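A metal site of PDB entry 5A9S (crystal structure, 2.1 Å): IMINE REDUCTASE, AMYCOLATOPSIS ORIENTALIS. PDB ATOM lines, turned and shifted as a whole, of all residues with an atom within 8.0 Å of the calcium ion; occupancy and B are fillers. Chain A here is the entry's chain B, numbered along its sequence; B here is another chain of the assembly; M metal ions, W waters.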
ATOM      1  N   GLN A 217      27.089  -5.380  28.415  1.00  0.00           N
ATOM      2  CA  GLN A 217      28.401  -4.764  28.217  1.00  0.00           C
ATOM      3  C   GLN A 217      28.299  -3.379  27.623  1.00  0.00           C
ATOM      4  O   GLN A 217      29.022  -2.486  28.033  1.00  0.00           O
ATOM      5  CB  GLN A 217      29.265  -5.651  27.329  1.00  0.00           C
ATOM      6  CG  GLN A 217      29.444  -7.017  28.012  1.00  0.00           C
ATOM      7  CD  GLN A 217      30.660  -7.021  28.826  1.00  0.00           C
ATOM      8  OE1 GLN A 217      30.613  -6.670  30.021  1.00  0.00           O
ATOM      9  NE2 GLN A 217      31.809  -7.273  28.168  1.00  0.00           N
ATOM     10  N   ILE A 218      27.416  -3.196  26.645  1.00  0.00           N
ATOM     11  CA  ILE A 218      27.157  -1.888  26.118  1.00  0.00           C
ATOM     12  C   ILE A 218      26.586  -0.911  27.109  1.00  0.00           C
ATOM     13  O   ILE A 218      26.962   0.263  27.068  1.00  0.00           O
ATOM     14  CB  ILE A 218      26.307  -1.949  24.865  1.00  0.00           C
ATOM     15  CG1 ILE A 218      27.233  -2.349  23.714  1.00  0.00           C
ATOM     16  CG2 ILE A 218      25.742  -0.599  24.578  1.00  0.00           C
ATOM     17  CD1 ILE A 218      26.492  -2.959  22.573  1.00  0.00           C
ATOM     18  N   ILE A 219      25.689  -1.338  27.962  1.00  0.00           N
ATOM     19  CA  ILE A 219      25.211  -0.464  29.032  1.00  0.00           C
ATOM     20  C   ILE A 219      26.373  -0.049  29.913  1.00  0.00           C
ATOM     21  O   ILE A 219      26.560   1.130  30.184  1.00  0.00           O
ATOM     22  CB  ILE A 219      24.161  -1.146  29.873  1.00  0.00           C
ATOM     23  CG1 ILE A 219      22.845  -1.188  29.082  1.00  0.00           C
ATOM     24  CG2 ILE A 219      23.930  -0.388  31.196  1.00  0.00           C
ATOM     25  CD1 ILE A 219      21.770  -2.078  29.663  1.00  0.00           C
ATOM     26  N   LYS A 220      27.178  -1.018  30.376  1.00  0.00           N
ATOM     27  CA  LYS A 220      28.354  -0.667  31.200  1.00  0.00           C
ATOM     28  C   LYS A 220      29.381   0.193  30.452  1.00  0.00           C
ATOM     29  O   LYS A 220      29.952   1.090  31.045  1.00  0.00           O
ATOM     30  CB  LYS A 220      29.044  -1.876  31.698  1.00  0.00           C
ATOM     31  CG  LYS A 220      28.330  -2.572  32.829  1.00  0.00           C
ATOM     32  CD  LYS A 220      29.123  -3.823  33.065  1.00  0.00           C
ATOM     33  CE  LYS A 220      28.824  -4.503  34.348  1.00  0.00           C
ATOM     34  NZ  LYS A 220      29.352  -5.895  34.253  1.00  0.00           N
ATOM     35  N   ALA A 221      29.558  -0.006  29.146  1.00  0.00           N
ATOM     36  CA  ALA A 221      30.406   0.831  28.319  1.00  0.00           C
ATOM     37  C   ALA A 221      29.858   2.251  28.246  1.00  0.00           C
ATOM     38  O   ALA A 221      30.559   3.207  28.467  1.00  0.00           O
ATOM     39  CB  ALA A 221      30.564   0.252  26.892  1.00  0.00           C
ATOM     40  N   GLN A 222      28.571   2.394  28.008  1.00  0.00           N
ATOM     41  CA  GLN A 222      28.000   3.735  27.938  1.00  0.00           C
ATOM     42  C   GLN A 222      27.970   4.451  29.274  1.00  0.00           C
ATOM     43  O   GLN A 222      27.990   5.683  29.301  1.00  0.00           O
ATOM     44  CB  GLN A 222      26.562   3.692  27.365  1.00  0.00           C
ATOM     45  CG  GLN A 222      26.520   3.365  25.869  1.00  0.00           C
ATOM     46  CD  GLN A 222      27.147   4.464  25.026  1.00  0.00           C
ATOM     47  OE1 GLN A 222      27.863   4.200  24.029  1.00  0.00           O
ATOM     48  NE2 GLN A 222      26.909   5.683  25.418  1.00  0.00           N
ATOM     49  N   ALA A 223      27.871   3.711  30.392  1.00  0.00           N
ATOM     50  CA  ALA A 223      27.688   4.352  31.713  1.00  0.00           C
ATOM     51  C   ALA A 223      28.937   5.189  32.018  1.00  0.00           C
ATOM     52  O   ALA A 223      30.038   4.631  32.050  1.00  0.00           O
ATOM     53  CB  ALA A 223      27.473   3.324  32.803  1.00  0.00           C
ATOM     54  N   PRO A 224      28.788   6.507  32.192  1.00  0.00           N
ATOM     55  CA  PRO A 224      30.016   7.316  32.316  1.00  0.00           C
ATOM     56  C   PRO A 224      30.898   6.997  33.540  1.00  0.00           C
ATOM     57  O   PRO A 224      32.094   7.233  33.508  1.00  0.00           O
ATOM     58  CB  PRO A 224      29.494   8.747  32.329  1.00  0.00           C
ATOM     59  CG  PRO A 224      28.051   8.655  32.698  1.00  0.00           C
ATOM     60  CD  PRO A 224      27.570   7.341  32.164  1.00  0.00           C
ATOM     61  N   THR A 225      30.380   6.357  34.567  1.00  0.00           N
ATOM     62  CA  THR A 225      31.229   6.072  35.725  1.00  0.00           C
ATOM     63  C   THR A 225      31.598   4.625  35.860  1.00  0.00           C
ATOM     64  O   THR A 225      31.951   4.211  36.953  1.00  0.00           O
ATOM     65  CB  THR A 225      30.530   6.557  37.009  1.00  0.00           C
ATOM     66  OG1 THR A 225      29.256   5.933  37.127  1.00  0.00           O
ATOM     67  CG2 THR A 225      30.381   8.059  36.978  1.00  0.00           C
ATOM     68  N   ILE A 226      31.488   3.841  34.785  1.00  0.00           N
ATOM     69  CA  ILE A 226      32.027   2.467  34.818  1.00  0.00           C
ATOM     70  C   ILE A 226      33.103   2.353  33.755  1.00  0.00           C
ATOM     71  O   ILE A 226      32.883   2.715  32.638  1.00  0.00           O
ATOM     72  CB  ILE A 226      30.918   1.439  34.620  1.00  0.00           C
ATOM     73  CG1 ILE A 226      30.004   1.500  35.846  1.00  0.00           C
ATOM     74  CG2 ILE A 226      31.537   0.029  34.437  1.00  0.00           C
ATOM     75  CD1 ILE A 226      28.844   0.571  35.766  1.00  0.00           C
ATOM     76  N   ASP A 227      34.266   1.835  34.133  1.00  0.00           N
ATOM     77  CA  ASP A 227      35.380   1.681  33.208  1.00  0.00           C
ATOM     78  C   ASP A 227      36.117   0.405  33.497  1.00  0.00           C
ATOM     79  O   ASP A 227      37.179   0.275  32.958  1.00  0.00           O
ATOM     80  CB  ASP A 227      36.323   2.868  33.344  1.00  0.00           C
ATOM     81  N   TYR A 231      35.821  -4.643  27.707  1.00  0.00           N
ATOM     82  CA  TYR A 231      34.992  -4.210  26.564  1.00  0.00           C
ATOM     83  C   TYR A 231      35.421  -2.835  26.046  1.00  0.00           C
ATOM     84  O   TYR A 231      35.243  -1.853  26.763  1.00  0.00           O
ATOM     85  CB  TYR A 231      33.502  -4.179  26.944  1.00  0.00           C
ATOM     86  CG  TYR A 231      32.543  -4.167  25.758  1.00  0.00           C
ATOM     87  CD1 TYR A 231      32.252  -5.337  25.044  1.00  0.00           C
ATOM     88  CD2 TYR A 231      31.912  -2.990  25.358  1.00  0.00           C
ATOM     89  CE1 TYR A 231      31.367  -5.326  23.959  1.00  0.00           C
ATOM     90  CE2 TYR A 231      31.033  -2.963  24.275  1.00  0.00           C
ATOM     91  CZ  TYR A 231      30.759  -4.137  23.585  1.00  0.00           C
ATOM     92  OH  TYR A 231      29.896  -4.141  22.543  1.00  0.00           O
ATOM     93  N   GLY A 233      34.583  -0.643  22.895  1.00  0.00           N
ATOM     94  CA  GLY A 233      33.707  -0.641  24.038  1.00  0.00           C
ATOM     95  C   GLY A 233      32.818   0.556  23.934  1.00  0.00           C
ATOM     96  O   GLY A 233      33.064   1.566  24.608  1.00  0.00           O
ATOM     97  N   ASP A 234      31.787   0.465  23.095  1.00  0.00           N
ATOM     98  CA  ASP A 234      30.877   1.596  22.869  1.00  0.00           C
ATOM     99  C   ASP A 234      29.620   1.276  22.043  1.00  0.00           C
ATOM    100  O   ASP A 234      29.760   0.522  21.097  1.00  0.00           O
ATOM    101  CB  ASP A 234      31.656   2.632  22.032  1.00  0.00           C
ATOM    102  CG  ASP A 234      31.275   4.028  22.337  1.00  0.00           C
ATOM    103  OD1 ASP A 234      31.433   4.422  23.504  1.00  0.00           O
ATOM    104  OD2 ASP A 234      30.837   4.724  21.407  1.00  0.00           O
ATOM    105  N   TYR A 283      24.432   7.500  25.790  1.00  0.00           N
ATOM    106  CA  TYR A 283      23.965   7.742  27.159  1.00  0.00           C
ATOM    107  C   TYR A 283      23.266   9.082  27.331  1.00  0.00           C
ATOM    108  O   TYR A 283      22.363   9.201  28.171  1.00  0.00           O
ATOM    109  CB  TYR A 283      25.118   7.652  28.133  1.00  0.00           C
ATOM    110  CG  TYR A 283      24.660   7.373  29.559  1.00  0.00           C
ATOM    111  CD1 TYR A 283      24.541   6.048  30.014  1.00  0.00           C
ATOM    112  CD2 TYR A 283      24.449   8.399  30.474  1.00  0.00           C
ATOM    113  CE1 TYR A 283      24.144   5.777  31.290  1.00  0.00           C
ATOM    114  CE2 TYR A 283      24.047   8.133  31.783  1.00  0.00           C
ATOM    115  CZ  TYR A 283      23.870   6.822  32.175  1.00  0.00           C
ATOM    116  OH  TYR A 283      23.513   6.520  33.456  1.00  0.00           O
ATOM    117  N   THR B 203      23.980   0.559  38.235  1.00  0.00           N
ATOM    118  CA  THR B 203      24.217  -0.032  36.927  1.00  0.00           C
ATOM    119  C   THR B 203      24.687  -1.468  37.062  1.00  0.00           C
ATOM    120  O   THR B 203      24.264  -2.332  36.311  1.00  0.00           O
ATOM    121  CB  THR B 203      25.195   0.817  36.084  1.00  0.00           C
ATOM    122  OG1 THR B 203      24.631   2.139  35.873  1.00  0.00           O
ATOM    123  CG2 THR B 203      25.441   0.185  34.719  1.00  0.00           C
HETATM  124 CA    CA M   1      31.546   3.186  30.849  1.00  0.00          CA
HETATM  125  O   HOH W   1      32.885   5.323  30.025  1.00  0.00           O
HETATM  126  O   HOH W   2      33.569   1.734  29.654  1.00  0.00           O
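The backbone carbonyl oxygen (O) of Ile 226 is bound to the calcium ion, at 2.3 Å.
O of Ala 223 binds the calcium ion (2.4 Å).
O of Ala 221 binds the calcium ion, 2.6 Å away.
O of Lys 220 binds the calcium ion (2.6 Å).
The calcium ion is bound by water W1.
Water W2 is bound to the calcium ion (2.8 Å).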
